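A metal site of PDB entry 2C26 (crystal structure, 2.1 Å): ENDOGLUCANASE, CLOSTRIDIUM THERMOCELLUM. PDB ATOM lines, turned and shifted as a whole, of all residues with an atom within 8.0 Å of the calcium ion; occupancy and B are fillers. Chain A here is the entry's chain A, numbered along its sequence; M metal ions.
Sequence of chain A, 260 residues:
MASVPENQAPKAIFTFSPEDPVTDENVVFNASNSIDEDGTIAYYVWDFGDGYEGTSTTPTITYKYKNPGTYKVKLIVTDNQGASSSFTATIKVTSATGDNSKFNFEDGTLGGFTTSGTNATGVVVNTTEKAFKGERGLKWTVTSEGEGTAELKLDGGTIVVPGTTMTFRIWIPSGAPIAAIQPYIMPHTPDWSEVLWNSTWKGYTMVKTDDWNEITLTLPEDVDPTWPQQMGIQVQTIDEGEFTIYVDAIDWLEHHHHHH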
ATOM      1  N   GLY A  98     -16.153  -8.213   2.086  1.00  0.00           N
ATOM      2  CA  GLY A  98     -15.403  -9.469   2.044  1.00  0.00           C
ATOM      3  C   GLY A  98     -15.680 -10.305   0.813  1.00  0.00           C
ATOM      4  O   GLY A  98     -16.382  -9.876  -0.113  1.00  0.00           O
ATOM      5  N   ASP A  99     -15.152 -11.528   0.814  1.00  0.00           N
ATOM      6  CA  ASP A  99     -15.109 -12.364  -0.383  1.00  0.00           C
ATOM      7  C   ASP A  99     -15.088 -13.837  -0.009  1.00  0.00           C
ATOM      8  O   ASP A  99     -14.115 -14.333   0.579  1.00  0.00           O
ATOM      9  CB  ASP A  99     -13.852 -12.015  -1.184  1.00  0.00           C
ATOM     10  CG  ASP A  99     -13.788 -12.707  -2.549  1.00  0.00           C
ATOM     11  OD1 ASP A  99     -14.672 -13.517  -2.888  1.00  0.00           O
ATOM     12  OD2 ASP A  99     -12.835 -12.406  -3.283  1.00  0.00           O
ATOM     13  N   ASN A 100     -16.166 -14.545  -0.372  1.00  0.00           N
ATOM     14  CA  ASN A 100     -16.357 -15.954  -0.047  1.00  0.00           C
ATOM     15  C   ASN A 100     -15.911 -16.928  -1.125  1.00  0.00           C
ATOM     16  O   ASN A 100     -16.127 -18.143  -1.002  1.00  0.00           O
ATOM     17  CB  ASN A 100     -17.825 -16.230   0.313  1.00  0.00           C
ATOM     18  CG  ASN A 100     -18.292 -15.450   1.532  1.00  0.00           C
ATOM     19  OD1 ASN A 100     -19.478 -15.134   1.657  1.00  0.00           O
ATOM     20  ND2 ASN A 100     -17.358 -15.127   2.432  1.00  0.00           N
ATOM     21  N   SER A 101     -15.292 -16.403  -2.187  1.00  0.00           N
ATOM     22  CA  SER A 101     -14.777 -17.199  -3.306  1.00  0.00           C
ATOM     23  C   SER A 101     -13.808 -18.254  -2.826  1.00  0.00           C
ATOM     24  O   SER A 101     -13.104 -18.049  -1.839  1.00  0.00           O
ATOM     25  CB  SER A 101     -14.047 -16.301  -4.300  1.00  0.00           C
ATOM     26  OG  SER A 101     -14.900 -15.282  -4.787  1.00  0.00           O
ATOM     27  N   PHE A 103     -11.015 -18.982  -4.180  1.00  0.00           N
ATOM     28  CA  PHE A 103      -9.788 -18.178  -4.147  1.00  0.00           C
ATOM     29  C   PHE A 103     -10.203 -16.724  -4.077  1.00  0.00           C
ATOM     30  O   PHE A 103     -10.605 -16.131  -5.075  1.00  0.00           O
ATOM     31  CB  PHE A 103      -8.895 -18.448  -5.366  1.00  0.00           C
ATOM     32  CG  PHE A 103      -8.260 -19.803  -5.345  1.00  0.00           C
ATOM     33  CD1 PHE A 103      -7.139 -20.052  -4.559  1.00  0.00           C
ATOM     34  CD2 PHE A 103      -8.779 -20.845  -6.110  1.00  0.00           C
ATOM     35  CE1 PHE A 103      -6.563 -21.312  -4.529  1.00  0.00           C
ATOM     36  CE2 PHE A 103      -8.198 -22.103  -6.093  1.00  0.00           C
ATOM     37  CZ  PHE A 103      -7.092 -22.337  -5.296  1.00  0.00           C
ATOM     38  N   ASN A 104     -10.097 -16.172  -2.868  1.00  0.00           N
ATOM     39  CA  ASN A 104     -10.591 -14.831  -2.565  1.00  0.00           C
ATOM     40  C   ASN A 104      -9.464 -13.842  -2.271  1.00  0.00           C
ATOM     41  O   ASN A 104      -9.650 -12.624  -2.367  1.00  0.00           O
ATOM     42  CB  ASN A 104     -11.596 -14.887  -1.419  1.00  0.00           C
ATOM     43  CG  ASN A 104     -11.038 -15.549  -0.151  1.00  0.00           C
ATOM     44  OD1 ASN A 104     -10.139 -15.031   0.506  1.00  0.00           O
ATOM     45  ND2 ASN A 104     -11.599 -16.699   0.192  1.00  0.00           N
ATOM     46  N   PHE A 105      -8.310 -14.393  -1.872  1.00  0.00           N
ATOM     47  CA  PHE A 105      -7.054 -13.652  -1.637  1.00  0.00           C
ATOM     48  C   PHE A 105      -7.109 -12.641  -0.496  1.00  0.00           C
ATOM     49  O   PHE A 105      -6.261 -11.745  -0.418  1.00  0.00           O
ATOM     50  CB  PHE A 105      -6.530 -13.039  -2.952  1.00  0.00           C
ATOM     51  CG  PHE A 105      -6.364 -14.061  -4.062  1.00  0.00           C
ATOM     52  CD1 PHE A 105      -5.296 -14.950  -4.051  1.00  0.00           C
ATOM     53  CD2 PHE A 105      -7.302 -14.131  -5.092  1.00  0.00           C
ATOM     54  CE1 PHE A 105      -5.154 -15.903  -5.065  1.00  0.00           C
ATOM     55  CE2 PHE A 105      -7.166 -15.076  -6.106  1.00  0.00           C
ATOM     56  CZ  PHE A 105      -6.094 -15.962  -6.086  1.00  0.00           C
ATOM     57  N   GLU A 106      -8.085 -12.818   0.393  1.00  0.00           N
ATOM     58  CA  GLU A 106      -8.290 -11.913   1.523  1.00  0.00           C
ATOM     59  C   GLU A 106      -7.278 -12.078   2.663  1.00  0.00           C
ATOM     60  O   GLU A 106      -7.087 -11.161   3.462  1.00  0.00           O
ATOM     61  CB  GLU A 106      -9.723 -12.059   2.081  1.00  0.00           C
ATOM     62  CG  GLU A 106     -10.835 -11.747   1.093  1.00  0.00           C
ATOM     63  CD  GLU A 106     -10.678 -10.380   0.426  1.00  0.00           C
ATOM     64  OE1 GLU A 106     -10.477  -9.363   1.132  1.00  0.00           O
ATOM     65  OE2 GLU A 106     -10.755 -10.328  -0.822  1.00  0.00           O
ATOM     66  N   ASP A 107      -6.618 -13.235   2.718  1.00  0.00           N
ATOM     67  CA  ASP A 107      -5.592 -13.478   3.735  1.00  0.00           C
ATOM     68  C   ASP A 107      -4.245 -12.810   3.429  1.00  0.00           C
ATOM     69  O   ASP A 107      -3.295 -12.927   4.218  1.00  0.00           O
ATOM     70  CB  ASP A 107      -5.420 -14.978   4.011  1.00  0.00           C
ATOM     71  CG  ASP A 107      -4.962 -15.752   2.782  1.00  0.00           C
ATOM     72  OD1 ASP A 107      -4.570 -15.135   1.767  1.00  0.00           O
ATOM     73  OD2 ASP A 107      -5.016 -17.005   2.839  1.00  0.00           O
ATOM     74  N   ASN A 126      -0.090 -10.200  -4.056  1.00  0.00           N
ATOM     75  CA  ASN A 126      -1.377  -9.920  -3.449  1.00  0.00           C
ATOM     76  C   ASN A 126      -1.533  -8.403  -3.302  1.00  0.00           C
ATOM     77  O   ASN A 126      -0.667  -7.737  -2.718  1.00  0.00           O
ATOM     78  CB  ASN A 126      -1.499 -10.648  -2.112  1.00  0.00           C
ATOM     79  CG  ASN A 126      -2.892 -10.579  -1.541  1.00  0.00           C
ATOM     80  OD1 ASN A 126      -3.304  -9.550  -1.027  1.00  0.00           O
ATOM     81  ND2 ASN A 126      -3.626 -11.678  -1.634  1.00  0.00           N
ATOM     82  N   THR A 127      -2.631  -7.870  -3.826  1.00  0.00           N
ATOM     83  CA  THR A 127      -2.819  -6.409  -3.960  1.00  0.00           C
ATOM     84  C   THR A 127      -4.137  -5.901  -3.365  1.00  0.00           C
ATOM     85  O   THR A 127      -5.118  -6.638  -3.317  1.00  0.00           O
ATOM     86  CB  THR A 127      -2.742  -5.975  -5.447  1.00  0.00           C
ATOM     87  OG1 THR A 127      -2.729  -4.552  -5.549  1.00  0.00           O
ATOM     88  CG2 THR A 127      -3.937  -6.518  -6.260  1.00  0.00           C
ATOM     89  N   LYS A 130      -6.777  -3.197  -6.899  1.00  0.00           N
ATOM     90  CA  LYS A 130      -8.034  -3.630  -7.482  1.00  0.00           C
ATOM     91  C   LYS A 130      -8.393  -4.991  -6.904  1.00  0.00           C
ATOM     92  O   LYS A 130      -7.500  -5.827  -6.650  1.00  0.00           O
ATOM     93  CB  LYS A 130      -7.948  -3.772  -8.999  1.00  0.00           C
ATOM     94  CG  LYS A 130      -8.011  -2.495  -9.770  1.00  0.00           C
ATOM     95  CD  LYS A 130      -7.976  -2.795 -11.259  1.00  0.00           C
ATOM     96  CE  LYS A 130      -7.286  -1.681 -12.035  1.00  0.00           C
ATOM     97  NZ  LYS A 130      -8.011  -0.390 -11.935  1.00  0.00           N
ATOM     98  N   ALA A 131      -9.688  -5.207  -6.725  1.00  0.00           N
ATOM     99  CA  ALA A 131     -10.248  -6.490  -6.326  1.00  0.00           C
ATOM    100  C   ALA A 131     -11.606  -6.586  -7.012  1.00  0.00           C
ATOM    101  O   ALA A 131     -12.192  -5.551  -7.362  1.00  0.00           O
ATOM    102  CB  ALA A 131     -10.401  -6.555  -4.816  1.00  0.00           C
ATOM    103  N   PHE A 132     -12.079  -7.802  -7.233  1.00  0.00           N
ATOM    104  CA  PHE A 132     -13.451  -8.021  -7.716  1.00  0.00           C
ATOM    105  C   PHE A 132     -14.432  -8.117  -6.542  1.00  0.00           C
ATOM    106  O   PHE A 132     -15.511  -7.532  -6.579  1.00  0.00           O
ATOM    107  CB  PHE A 132     -13.542  -9.247  -8.645  1.00  0.00           C
ATOM    108  CG  PHE A 132     -14.904  -9.431  -9.266  1.00  0.00           C
ATOM    109  CD1 PHE A 132     -15.267  -8.726 -10.404  1.00  0.00           C
ATOM    110  CD2 PHE A 132     -15.822 -10.310  -8.702  1.00  0.00           C
ATOM    111  CE1 PHE A 132     -16.533  -8.881 -10.980  1.00  0.00           C
ATOM    112  CE2 PHE A 132     -17.083 -10.483  -9.262  1.00  0.00           C
ATOM    113  CZ  PHE A 132     -17.443  -9.766 -10.406  1.00  0.00           C
ATOM    114  N   LYS A 133     -14.059  -8.876  -5.511  1.00  0.00           N
ATOM    115  CA  LYS A 133     -14.828  -8.952  -4.272  1.00  0.00           C
ATOM    116  C   LYS A 133     -13.910  -8.764  -3.065  1.00  0.00           C
ATOM    117  O   LYS A 133     -12.746  -9.166  -3.109  1.00  0.00           O
ATOM    118  CB  LYS A 133     -15.547 -10.297  -4.141  1.00  0.00           C
ATOM    119  CG  LYS A 133     -16.794 -10.464  -4.998  1.00  0.00           C
ATOM    120  CD  LYS A 133     -17.329 -11.894  -4.846  1.00  0.00           C
ATOM    121  CE  LYS A 133     -18.420 -12.211  -5.871  1.00  0.00           C
ATOM    122  NZ  LYS A 133     -19.211 -13.425  -5.482  1.00  0.00           N
ATOM    123  N   GLY A 134     -14.440  -8.162  -2.007  1.00  0.00           N
ATOM    124  CA  GLY A 134     -13.632  -7.879  -0.816  1.00  0.00           C
ATOM    125  C   GLY A 134     -12.588  -6.825  -1.083  1.00  0.00           C
ATOM    126  O   GLY A 134     -12.767  -5.961  -1.950  1.00  0.00           O
ATOM    127  N   GLU A 135     -11.479  -6.900  -0.352  1.00  0.00           N
ATOM    128  CA  GLU A 135     -10.445  -5.881  -0.392  1.00  0.00           C
ATOM    129  C   GLU A 135      -9.193  -6.267  -1.195  1.00  0.00           C
ATOM    130  O   GLU A 135      -8.414  -5.391  -1.576  1.00  0.00           O
ATOM    131  CB  GLU A 135     -10.021  -5.497   1.032  1.00  0.00           C
ATOM    132  CG  GLU A 135     -11.098  -4.757   1.820  1.00  0.00           C
ATOM    133  CD  GLU A 135     -10.525  -4.016   3.014  1.00  0.00           C
ATOM    134  OE1 GLU A 135      -9.419  -3.425   2.884  1.00  0.00           O
ATOM    135  OE2 GLU A 135     -11.179  -4.008   4.083  1.00  0.00           O
ATOM    136  N   ARG A 136      -9.003  -7.552  -1.445  1.00  0.00           N
ATOM    137  CA  ARG A 136      -7.745  -8.043  -1.992  1.00  0.00           C
ATOM    138  C   ARG A 136      -7.908  -8.927  -3.223  1.00  0.00           C
ATOM    139  O   ARG A 136      -8.939  -9.592  -3.384  1.00  0.00           O
ATOM    140  CB  ARG A 136      -6.941  -8.755  -0.904  1.00  0.00           C
ATOM    141  CG  ARG A 136      -6.353  -7.820   0.163  1.00  0.00           C
ATOM    142  CD  ARG A 136      -5.453  -8.571   1.131  1.00  0.00           C
ATOM    143  NE  ARG A 136      -4.729  -7.670   2.018  1.00  0.00           N
ATOM    144  CZ  ARG A 136      -3.533  -7.125   1.750  1.00  0.00           C
ATOM    145  NH1 ARG A 136      -2.907  -7.384   0.609  1.00  0.00           N
ATOM    146  NH2 ARG A 136      -2.966  -6.320   2.646  1.00  0.00           N
ATOM    147  N   GLY A 137      -6.897  -8.926  -4.086  1.00  0.00           N
ATOM    148  CA  GLY A 137      -6.868  -9.792  -5.269  1.00  0.00           C
ATOM    149  C   GLY A 137      -5.423 -10.084  -5.615  1.00  0.00           C
ATOM    150  O   GLY A 137      -4.530  -9.845  -4.805  1.00  0.00           O
ATOM    151  N   LEU A 138      -5.190 -10.604  -6.819  1.00  0.00           N
ATOM    152  CA  LEU A 138      -3.835 -10.750  -7.351  1.00  0.00           C
ATOM    153  C   LEU A 138      -3.557  -9.690  -8.411  1.00  0.00           C
ATOM    154  O   LEU A 138      -4.439  -9.316  -9.189  1.00  0.00           O
ATOM    155  CB  LEU A 138      -3.590 -12.138  -7.930  1.00  0.00           C
ATOM    156  CG  LEU A 138      -3.596 -13.368  -7.006  1.00  0.00           C
ATOM    157  CD1 LEU A 138      -3.307 -14.620  -7.835  1.00  0.00           C
ATOM    158  CD2 LEU A 138      -2.599 -13.246  -5.859  1.00  0.00           C
ATOM    159  N   TRP A 212     -13.349  -5.612 -15.605  1.00  0.00           N
ATOM    160  CA  TRP A 212     -13.430  -6.999 -15.170  1.00  0.00           C
ATOM    161  C   TRP A 212     -14.156  -7.848 -16.196  1.00  0.00           C
ATOM    162  O   TRP A 212     -15.194  -7.455 -16.727  1.00  0.00           O
ATOM    163  CB  TRP A 212     -14.133  -7.101 -13.812  1.00  0.00           C
ATOM    164  CG  TRP A 212     -13.292  -6.606 -12.694  1.00  0.00           C
ATOM    165  CD1 TRP A 212     -13.410  -5.412 -12.026  1.00  0.00           C
ATOM    166  CD2 TRP A 212     -12.178  -7.296 -12.088  1.00  0.00           C
ATOM    167  NE1 TRP A 212     -12.439  -5.316 -11.050  1.00  0.00           N
ATOM    168  CE2 TRP A 212     -11.669  -6.452 -11.074  1.00  0.00           C
ATOM    169  CE3 TRP A 212     -11.566  -8.533 -12.322  1.00  0.00           C
ATOM    170  CZ2 TRP A 212     -10.571  -6.809 -10.276  1.00  0.00           C
ATOM    171  CZ3 TRP A 212     -10.472  -8.893 -11.533  1.00  0.00           C
ATOM    172  CH2 TRP A 212      -9.987  -8.028 -10.518  1.00  0.00           C
ATOM    173  N   VAL A 247      -6.462 -10.452 -11.124  1.00  0.00           N
ATOM    174  CA  VAL A 247      -7.220 -11.683 -11.019  1.00  0.00           C
ATOM    175  C   VAL A 247      -7.757 -11.793  -9.593  1.00  0.00           C
ATOM    176  O   VAL A 247      -7.015 -11.615  -8.632  1.00  0.00           O
ATOM    177  CB  VAL A 247      -6.343 -12.911 -11.359  1.00  0.00           C
ATOM    178  CG1 VAL A 247      -7.115 -14.213 -11.191  1.00  0.00           C
ATOM    179  CG2 VAL A 247      -5.768 -12.802 -12.786  1.00  0.00           C
ATOM    180  N   ASP A 248      -9.044 -12.082  -9.471  1.00  0.00           N
ATOM    181  CA  ASP A 248      -9.670 -12.239  -8.165  1.00  0.00           C
ATOM    182  C   ASP A 248     -10.886 -13.171  -8.236  1.00  0.00           C
ATOM    183  O   ASP A 248     -11.413 -13.445  -9.317  1.00  0.00           O
ATOM    184  CB  ASP A 248     -10.091 -10.866  -7.598  1.00  0.00           C
ATOM    185  CG  ASP A 248     -10.505 -10.931  -6.131  1.00  0.00           C
ATOM    186  OD1 ASP A 248     -10.101 -11.905  -5.449  1.00  0.00           O
ATOM    187  OD2 ASP A 248     -11.221 -10.021  -5.649  1.00  0.00           O
ATOM    188  N   ALA A 249     -11.306 -13.656  -7.068  1.00  0.00           N
ATOM    189  CA  ALA A 249     -12.586 -14.314  -6.910  1.00  0.00           C
ATOM    190  C   ALA A 249     -12.804 -15.460  -7.900  1.00  0.00           C
ATOM    191  O   ALA A 249     -13.850 -15.560  -8.549  1.00  0.00           O
ATOM    192  CB  ALA A 249     -13.745 -13.276  -6.986  1.00  0.00           C
ATOM    193  N   ILE A 250     -11.807 -16.339  -8.013  1.00  0.00           N
ATOM    194  CA  ILE A 250     -11.966 -17.602  -8.727  1.00  0.00           C
ATOM    195  C   ILE A 250     -12.846 -18.488  -7.840  1.00  0.00           C
ATOM    196  O   ILE A 250     -12.551 -18.686  -6.663  1.00  0.00           O
ATOM    197  CB  ILE A 250     -10.621 -18.285  -9.072  1.00  0.00           C
ATOM    198  CG1 ILE A 250      -9.747 -17.338  -9.910  1.00  0.00           C
ATOM    199  CG2 ILE A 250     -10.895 -19.580  -9.846  1.00  0.00           C
ATOM    200  CD1 ILE A 250      -8.293 -17.758 -10.015  1.00  0.00           C
HETATM  201 CA    CA M   1     -10.921 -10.805  -3.271  1.00  0.00          CA
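OE1 of Glu 106 is in hydrogen-bond range of N of Glu 135 (3.0 Å). The side-chain carboxylate (OD2) of Asp 248 lies close to the backbone NH (N) of Phe 132 (2.9 Å). The side-chain amide nitrogen of Asn 104 lies within hydrogen-bond range of the backbone carbonyl oxygen of Ser 101. The side-chain carboxylate of Asp 99 sits at hydrogen-bond distance from the side-chain hydroxyl of Ser 101, 2.6 Å away. The side-chain amide oxygen (OD1) of Asn 126 sits at hydrogen-bond distance from the guanidinium group (NH1) of Arg 136 (2.7 Å).
Within 4 Å of the calcium ion: Asp 99, Asn 104, Glu 106, Lys 133, Arg 136 and Asp 248.
O of Arg 136 is bound to the calcium ion (2.3 Å). O of Asn 104 is bound to the calcium ion, at 2.4 Å. The calcium ion is bound by O of Lys 133 (2.5 Å). OD2 of Asp 99 binds the calcium ion (2.5 Å). The calcium ion is bound by OE2 of Glu 106 (2.5 Å). The calcium ion is bound by OD2 of Asp 248, at 2.5 Å. OD1 of Asp 248 binds the calcium ion (2.6 Å). The calcium ion has seven donor atoms within binding distance.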
